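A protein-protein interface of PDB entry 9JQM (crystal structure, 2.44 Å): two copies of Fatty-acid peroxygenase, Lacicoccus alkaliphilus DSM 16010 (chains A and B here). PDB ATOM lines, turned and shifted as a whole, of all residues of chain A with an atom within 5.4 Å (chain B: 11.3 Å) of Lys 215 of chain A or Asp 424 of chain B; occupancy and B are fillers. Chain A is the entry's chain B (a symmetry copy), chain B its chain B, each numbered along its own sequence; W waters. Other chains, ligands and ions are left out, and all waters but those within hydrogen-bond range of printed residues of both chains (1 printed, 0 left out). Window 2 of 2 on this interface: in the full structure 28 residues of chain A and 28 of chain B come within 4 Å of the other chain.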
ATOM      1  N   THR A 106     -10.884  -8.952 -12.480  1.00  0.00           N
ATOM      2  CA  THR A 106      -9.715  -9.804 -12.332  1.00  0.00           C
ATOM      3  C   THR A 106      -9.861 -10.719 -11.120  1.00  0.00           C
ATOM      4  O   THR A 106     -10.611 -10.436 -10.173  1.00  0.00           O
ATOM      5  CB  THR A 106      -8.443  -8.972 -12.194  1.00  0.00           C
ATOM      6  OG1 THR A 106      -8.462  -8.281 -10.935  1.00  0.00           O
ATOM      7  CG2 THR A 106      -8.321  -7.962 -13.327  1.00  0.00           C
ATOM      8  N   PRO A 213      -7.015   7.308  -5.848  1.00  0.00           N
ATOM      9  CA  PRO A 213      -7.560   5.968  -5.715  1.00  0.00           C
ATOM     10  C   PRO A 213      -6.515   4.938  -6.100  1.00  0.00           C
ATOM     11  O   PRO A 213      -5.651   5.200  -6.953  1.00  0.00           O
ATOM     12  CB  PRO A 213      -8.740   5.969  -6.697  1.00  0.00           C
ATOM     13  CG  PRO A 213      -8.391   7.011  -7.697  1.00  0.00           C
ATOM     14  CD  PRO A 213      -7.719   8.085  -6.886  1.00  0.00           C
ATOM     15  N   PRO A 214      -6.548   3.763  -5.484  1.00  0.00           N
ATOM     16  CA  PRO A 214      -5.604   2.699  -5.853  1.00  0.00           C
ATOM     17  C   PRO A 214      -5.741   2.286  -7.311  1.00  0.00           C
ATOM     18  O   PRO A 214      -6.848   2.159  -7.842  1.00  0.00           O
ATOM     19  CB  PRO A 214      -5.988   1.546  -4.918  1.00  0.00           C
ATOM     20  CG  PRO A 214      -6.705   2.193  -3.772  1.00  0.00           C
ATOM     21  CD  PRO A 214      -7.403   3.393  -4.348  1.00  0.00           C
ATOM     22  N   LYS A 215      -4.600   2.069  -7.959  1.00  0.00           N
ATOM     23  CA  LYS A 215      -4.606   1.501  -9.302  1.00  0.00           C
ATOM     24  C   LYS A 215      -5.394   0.196  -9.313  1.00  0.00           C
ATOM     25  O   LYS A 215      -5.295  -0.614  -8.387  1.00  0.00           O
ATOM     26  CB  LYS A 215      -3.178   1.261  -9.792  1.00  0.00           C
ATOM     27  CG  LYS A 215      -3.111   0.734 -11.219  1.00  0.00           C
ATOM     28  CD  LYS A 215      -1.862  -0.124 -11.459  1.00  0.00           C
ATOM     29  CE  LYS A 215      -1.722  -1.238 -10.410  1.00  0.00           C
ATOM     30  NZ  LYS A 215      -2.745  -2.332 -10.539  1.00  0.00           N
ATOM     31  N   GLY A 216      -6.221   0.021 -10.343  1.00  0.00           N
ATOM     32  CA  GLY A 216      -7.024  -1.173 -10.489  1.00  0.00           C
ATOM     33  C   GLY A 216      -8.440  -1.066  -9.956  1.00  0.00           C
ATOM     34  O   GLY A 216      -9.255  -1.943 -10.260  1.00  0.00           O
ATOM     35  N   THR A 217      -8.750  -0.050  -9.149  1.00  0.00           N
ATOM     36  CA  THR A 217     -10.129   0.162  -8.745  1.00  0.00           C
ATOM     37  C   THR A 217     -10.885   0.854  -9.865  1.00  0.00           C
ATOM     38  O   THR A 217     -10.297   1.547 -10.707  1.00  0.00           O
ATOM     39  CB  THR A 217     -10.250   0.995  -7.458  1.00  0.00           C
ATOM     40  OG1 THR A 217      -9.754   2.327  -7.674  1.00  0.00           O
ATOM     41  CG2 THR A 217      -9.519   0.346  -6.307  1.00  0.00           C
ATOM     42  N   TYR A 220     -10.117   4.630 -10.265  1.00  0.00           N
ATOM     43  CA  TYR A 220      -8.860   4.867 -10.962  1.00  0.00           C
ATOM     44  C   TYR A 220      -8.994   4.553 -12.446  1.00  0.00           C
ATOM     45  O   TYR A 220      -8.676   5.388 -13.301  1.00  0.00           O
ATOM     46  CB  TYR A 220      -7.731   4.033 -10.329  1.00  0.00           C
ATOM     47  CG  TYR A 220      -6.389   4.230 -11.004  1.00  0.00           C
ATOM     48  CD1 TYR A 220      -6.075   3.539 -12.173  1.00  0.00           C
ATOM     49  CD2 TYR A 220      -5.443   5.120 -10.489  1.00  0.00           C
ATOM     50  CE1 TYR A 220      -4.868   3.725 -12.815  1.00  0.00           C
ATOM     51  CE2 TYR A 220      -4.223   5.321 -11.126  1.00  0.00           C
ATOM     52  CZ  TYR A 220      -3.941   4.617 -12.293  1.00  0.00           C
ATOM     53  OH  TYR A 220      -2.741   4.779 -12.954  1.00  0.00           O
ATOM     54  N   GLU A 221      -9.436   3.328 -12.768  1.00  0.00           N
ATOM     55  CA  GLU A 221      -9.475   2.898 -14.161  1.00  0.00           C
ATOM     56  C   GLU A 221     -10.453   3.733 -14.981  1.00  0.00           C
ATOM     57  O   GLU A 221     -10.188   4.043 -16.145  1.00  0.00           O
ATOM     58  CB  GLU A 221      -9.843   1.423 -14.258  1.00  0.00           C
ATOM     59  CG  GLU A 221      -8.937   0.486 -13.476  1.00  0.00           C
ATOM     60  CD  GLU A 221      -7.470   0.589 -13.881  1.00  0.00           C
ATOM     61  OE1 GLU A 221      -7.182   0.733 -15.079  1.00  0.00           O
ATOM     62  OE2 GLU A 221      -6.597   0.508 -12.996  1.00  0.00           O
ATOM     63  N   GLU B 129      -5.968   4.565   6.829  1.00  0.00           N
ATOM     64  CA  GLU B 129      -5.679   5.247   5.571  1.00  0.00           C
ATOM     65  C   GLU B 129      -6.118   6.697   5.602  1.00  0.00           C
ATOM     66  O   GLU B 129      -5.558   7.526   4.886  1.00  0.00           O
ATOM     67  CB  GLU B 129      -6.382   4.568   4.405  1.00  0.00           C
ATOM     68  CG  GLU B 129      -5.751   3.310   3.882  1.00  0.00           C
ATOM     69  CD  GLU B 129      -6.534   2.762   2.692  1.00  0.00           C
ATOM     70  OE1 GLU B 129      -7.581   3.361   2.372  1.00  0.00           O
ATOM     71  OE2 GLU B 129      -6.120   1.748   2.080  1.00  0.00           O
ATOM     72  N   ARG B 418      -1.529   2.444   3.350  1.00  0.00           N
ATOM     73  CA  ARG B 418      -2.313   2.013   2.199  1.00  0.00           C
ATOM     74  C   ARG B 418      -2.423   0.500   2.183  1.00  0.00           C
ATOM     75  O   ARG B 418      -1.409  -0.200   2.262  1.00  0.00           O
ATOM     76  CB  ARG B 418      -1.697   2.495   0.881  1.00  0.00           C
ATOM     77  CG  ARG B 418      -1.779   4.015   0.673  1.00  0.00           C
ATOM     78  CD  ARG B 418      -3.181   4.484   0.217  1.00  0.00           C
ATOM     79  NE  ARG B 418      -3.159   4.827  -1.202  1.00  0.00           N
ATOM     80  CZ  ARG B 418      -4.222   5.107  -1.941  1.00  0.00           C
ATOM     81  NH1 ARG B 418      -5.445   5.129  -1.423  1.00  0.00           N
ATOM     82  NH2 ARG B 418      -4.055   5.376  -3.235  1.00  0.00           N
ATOM     83  N   GLU B 419      -3.651   0.004   2.075  1.00  0.00           N
ATOM     84  CA  GLU B 419      -3.872  -1.430   1.955  1.00  0.00           C
ATOM     85  C   GLU B 419      -3.115  -1.981   0.758  1.00  0.00           C
ATOM     86  O   GLU B 419      -2.885  -1.285  -0.233  1.00  0.00           O
ATOM     87  CB  GLU B 419      -5.364  -1.738   1.814  1.00  0.00           C
ATOM     88  CG  GLU B 419      -5.691  -3.201   1.952  1.00  0.00           C
ATOM     89  CD  GLU B 419      -7.138  -3.449   2.336  1.00  0.00           C
ATOM     90  OE1 GLU B 419      -7.978  -2.556   2.084  1.00  0.00           O
ATOM     91  OE2 GLU B 419      -7.435  -4.547   2.875  1.00  0.00           O
ATOM     92  N   VAL B 420      -2.719  -3.244   0.867  1.00  0.00           N
ATOM     93  CA  VAL B 420      -2.001  -3.956  -0.178  1.00  0.00           C
ATOM     94  C   VAL B 420      -3.004  -4.907  -0.813  1.00  0.00           C
ATOM     95  O   VAL B 420      -3.491  -5.834  -0.161  1.00  0.00           O
ATOM     96  CB  VAL B 420      -0.778  -4.705   0.389  1.00  0.00           C
ATOM     97  CG1 VAL B 420      -0.168  -5.632  -0.646  1.00  0.00           C
ATOM     98  CG2 VAL B 420       0.271  -3.721   0.913  1.00  0.00           C
ATOM     99  N   VAL B 421      -3.353  -4.658  -2.072  1.00  0.00           N
ATOM    100  CA  VAL B 421      -4.281  -5.510  -2.812  1.00  0.00           C
ATOM    101  C   VAL B 421      -3.741  -5.657  -4.222  1.00  0.00           C
ATOM    102  O   VAL B 421      -3.543  -4.657  -4.919  1.00  0.00           O
ATOM    103  CB  VAL B 421      -5.719  -4.949  -2.864  1.00  0.00           C
ATOM    104  CG1 VAL B 421      -6.675  -5.994  -3.450  1.00  0.00           C
ATOM    105  CG2 VAL B 421      -6.198  -4.533  -1.481  1.00  0.00           C
ATOM    106  N   ASP B 422      -3.537  -6.894  -4.652  1.00  0.00           N
ATOM    107  CA  ASP B 422      -3.100  -7.199  -6.013  1.00  0.00           C
ATOM    108  C   ASP B 422      -4.336  -7.272  -6.911  1.00  0.00           C
ATOM    109  O   ASP B 422      -4.890  -8.340  -7.161  1.00  0.00           O
ATOM    110  CB  ASP B 422      -2.310  -8.505  -6.027  1.00  0.00           C
ATOM    111  CG  ASP B 422      -1.536  -8.724  -7.324  1.00  0.00           C
ATOM    112  OD1 ASP B 422      -1.587  -7.850  -8.223  1.00  0.00           O
ATOM    113  OD2 ASP B 422      -0.867  -9.778  -7.442  1.00  0.00           O
ATOM    114  N   ARG B 423      -4.772  -6.119  -7.419  1.00  0.00           N
ATOM    115  CA  ARG B 423      -5.984  -6.071  -8.230  1.00  0.00           C
ATOM    116  C   ARG B 423      -5.751  -6.422  -9.699  1.00  0.00           C
ATOM    117  O   ARG B 423      -6.721  -6.651 -10.427  1.00  0.00           O
ATOM    118  CB  ARG B 423      -6.627  -4.684  -8.124  1.00  0.00           C
ATOM    119  CG  ARG B 423      -7.165  -4.344  -6.728  1.00  0.00           C
ATOM    120  CD  ARG B 423      -7.340  -2.847  -6.607  1.00  0.00           C
ATOM    121  NE  ARG B 423      -7.972  -2.454  -5.352  1.00  0.00           N
ATOM    122  CZ  ARG B 423      -7.319  -1.889  -4.343  1.00  0.00           C
ATOM    123  NH1 ARG B 423      -6.010  -1.661  -4.406  1.00  0.00           N
ATOM    124  NH2 ARG B 423      -7.987  -1.560  -3.241  1.00  0.00           N
ATOM    125  N   ASP B 424      -4.508  -6.468 -10.166  1.00  0.00           N
ATOM    126  CA  ASP B 424      -4.234  -6.833 -11.550  1.00  0.00           C
ATOM    127  C   ASP B 424      -3.751  -8.273 -11.691  1.00  0.00           C
ATOM    128  O   ASP B 424      -3.393  -8.690 -12.793  1.00  0.00           O
ATOM    129  CB  ASP B 424      -3.231  -5.857 -12.183  1.00  0.00           C
ATOM    130  CG  ASP B 424      -2.138  -5.413 -11.218  1.00  0.00           C
ATOM    131  OD1 ASP B 424      -1.254  -4.629 -11.637  1.00  0.00           O
ATOM    132  OD2 ASP B 424      -2.157  -5.840 -10.038  1.00  0.00           O
ATOM    133  N   LEU B 425      -3.727  -9.028 -10.598  1.00  0.00           N
ATOM    134  CA  LEU B 425      -3.542 -10.469 -10.629  1.00  0.00           C
ATOM    135  C   LEU B 425      -4.642 -11.117 -11.461  1.00  0.00           C
ATOM    136  O   LEU B 425      -5.800 -11.175 -11.036  1.00  0.00           O
ATOM    137  CB  LEU B 425      -3.546 -11.031  -9.204  1.00  0.00           C
ATOM    138  CG  LEU B 425      -3.596 -12.557  -9.036  1.00  0.00           C
ATOM    139  CD1 LEU B 425      -2.363 -13.212  -9.652  1.00  0.00           C
ATOM    140  CD2 LEU B 425      -3.742 -12.953  -7.575  1.00  0.00           C
ATOM    141  N   GLU B 426      -4.307 -11.576 -12.659  1.00  0.00           N
ATOM    142  CA  GLU B 426      -5.223 -12.373 -13.458  1.00  0.00           C
ATOM    143  C   GLU B 426      -4.769 -13.823 -13.437  1.00  0.00           C
ATOM    144  O   GLU B 426      -3.634 -14.133 -13.087  1.00  0.00           O
ATOM    145  CB  GLU B 426      -5.311 -11.853 -14.894  1.00  0.00           C
ATOM    146  CG  GLU B 426      -6.595 -11.070 -15.163  1.00  0.00           C
ATOM    147  CD  GLU B 426      -6.508 -10.169 -16.383  1.00  0.00           C
ATOM    148  OE1 GLU B 426      -7.553  -9.954 -17.049  1.00  0.00           O
ATOM    149  OE2 GLU B 426      -5.398  -9.659 -16.665  1.00  0.00           O
ATOM    150  N   HIS B 427      -5.671 -14.717 -13.803  1.00  0.00           N
ATOM    151  CA  HIS B 427      -5.310 -16.111 -13.650  1.00  0.00           C
ATOM    152  C   HIS B 427      -4.256 -16.576 -14.657  1.00  0.00           C
ATOM    153  O   HIS B 427      -3.859 -17.741 -14.579  1.00  0.00           O
ATOM    154  CB  HIS B 427      -6.566 -16.990 -13.708  1.00  0.00           C
ATOM    155  CG  HIS B 427      -6.546 -18.107 -12.708  1.00  0.00           C
ATOM    156  ND1 HIS B 427      -6.899 -17.931 -11.382  1.00  0.00           N
ATOM    157  CD2 HIS B 427      -6.211 -19.413 -12.842  1.00  0.00           C
ATOM    158  CE1 HIS B 427      -6.781 -19.083 -10.745  1.00  0.00           C
ATOM    159  NE2 HIS B 427      -6.367 -19.997 -11.607  1.00  0.00           N
ATOM    160  N   HIS B 428      -3.779 -15.710 -15.566  1.00  0.00           N
ATOM    161  CA  HIS B 428      -2.607 -16.031 -16.387  1.00  0.00           C
ATOM    162  C   HIS B 428      -1.292 -15.884 -15.627  1.00  0.00           C
ATOM    163  O   HIS B 428      -0.252 -16.263 -16.171  1.00  0.00           O
ATOM    164  CB  HIS B 428      -2.464 -15.124 -17.630  1.00  0.00           C
ATOM    165  CG  HIS B 428      -3.745 -14.558 -18.156  1.00  0.00           C
ATOM    166  ND1 HIS B 428      -3.953 -13.202 -18.295  1.00  0.00           N
ATOM    167  CD2 HIS B 428      -4.873 -15.162 -18.605  1.00  0.00           C
ATOM    168  CE1 HIS B 428      -5.163 -12.995 -18.786  1.00  0.00           C
ATOM    169  NE2 HIS B 428      -5.744 -14.167 -18.981  1.00  0.00           N
ATOM    170  N   HIS B 429      -1.294 -15.302 -14.424  1.00  0.00           N
ATOM    171  CA  HIS B 429      -0.046 -14.872 -13.780  1.00  0.00           C
ATOM    172  C   HIS B 429       0.493 -15.894 -12.771  1.00  0.00           C
ATOM    173  O   HIS B 429      -0.126 -16.174 -11.734  1.00  0.00           O
ATOM    174  CB  HIS B 429      -0.243 -13.506 -13.092  1.00  0.00           C
ATOM    175  CG  HIS B 429      -0.702 -12.412 -14.014  1.00  0.00           C
ATOM    176  ND1 HIS B 429      -1.356 -11.285 -13.562  1.00  0.00           N
ATOM    177  CD2 HIS B 429      -0.608 -12.275 -15.360  1.00  0.00           C
ATOM    178  CE1 HIS B 429      -1.636 -10.497 -14.588  1.00  0.00           C
ATOM    179  NE2 HIS B 429      -1.194 -11.075 -15.692  1.00  0.00           N
HETATM  180  O   HOH W   1      -3.909  -2.079  -6.344  1.00  0.00           O
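OG1 of Thr 106 of chain A is in hydrogen-bond range of O of Arg 423 of chain B (2.4 Å). OD1 of Asp 424 of chain B lies within salt-bridge range of NZ of Lys 215 of chain A, at 3.0 Å.
The backbone NH (N) of Leu 425 of chain B is in hydrogen-bond range of the side-chain carboxylate (OD1) of Asp 422 of chain B (3.4 Å). ND1 of His 429 of chain B lies close to O of Asp 424 of chain B (3.4 Å). O of Pro 214 of chain A lies within hydrogen-bond range of OG1 of Thr 217 of chain A. N of Gly 216 of chain A is in hydrogen-bond range of OE2 of Glu 221 of chain A. The side-chain hydroxyl (OG1) of Thr 217 of chain A is in hydrogen-bond range of the backbone NH (N) of Tyr 220 of chain A (3.5 Å).
CB of Thr 106 of chain A touches O of Leu 425 of chain B, at 3.6 Å. Pro 213 of chain A touches Arg 418 of chain B (C to NH2, 3.8 Å). Pro 214 of chain A touches Arg 418 of chain B. CB of Pro 214 of chain A touches NH1 of Arg 423 of chain B, at 3.2 Å. Arg 423 of chain B touches Lys 215 of chain A. C of Gly 216 of chain A touches CD of Arg 423 of chain B, 3.9 Å away. CG2 of Thr 217 of chain A touches NE of Arg 423 of chain B (3.3 Å).
Of chain B, only Arg 423 and Asp 424 come within 4 Å of Lys 215 of chain A. Asp 424 of chain B touches just one residue of chain A: Lys 215 (3.0 Å). Pro 213 of chain A touches just one residue of chain B: Arg 418 (3.8 Å). Of chain B, only Arg 418 and Arg 423 come within 4 Å of Pro 214 of chain A. Printed residues of chain A within 4 Å of Arg 423 of chain B: Thr 106, Pro 214, Lys 215, Gly 216 and Thr 217. Printed residues of chain B within 4 Å of Thr 106 of chain A: Arg 423 and Leu 425. Printed residues of chain A within 4 Å of Leu 425 of chain B: Thr 106. Of the printed residues of chain A, Arg 418 of chain B touches Pro 213 and Pro 214. The nearest printed residue of chain A that does not touch Arg 423 of chain B is Pro 213 of chain A (6.8 Å).
Along chain B the printed residues that touch a printed residue of chain A span positions 418 to 425. Hydrophobic or aromatic side chains of chain A within 4 Å of the printed part of chain B: Pro 214. Along chain A the printed residues that touch a printed residue of chain B span positions 106 to 217. Among the printed residues, 9 pairs touch across the chains. Among the printed residues, Asp or Glu carboxylates within 4 Å of a Lys or Arg side-chain nitrogen of the other chain: Lys 215 of chain A with Asp 424 of chain B (3.0 Å).
No position is printed for both chains.
Water W1 lies within hydrogen-bond range of O of Lys 215 of chain A (2.9 Å), NH1 of Arg 423 of chain B (2.9 Å) and O of Val 421 of chain B (3.0 Å).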
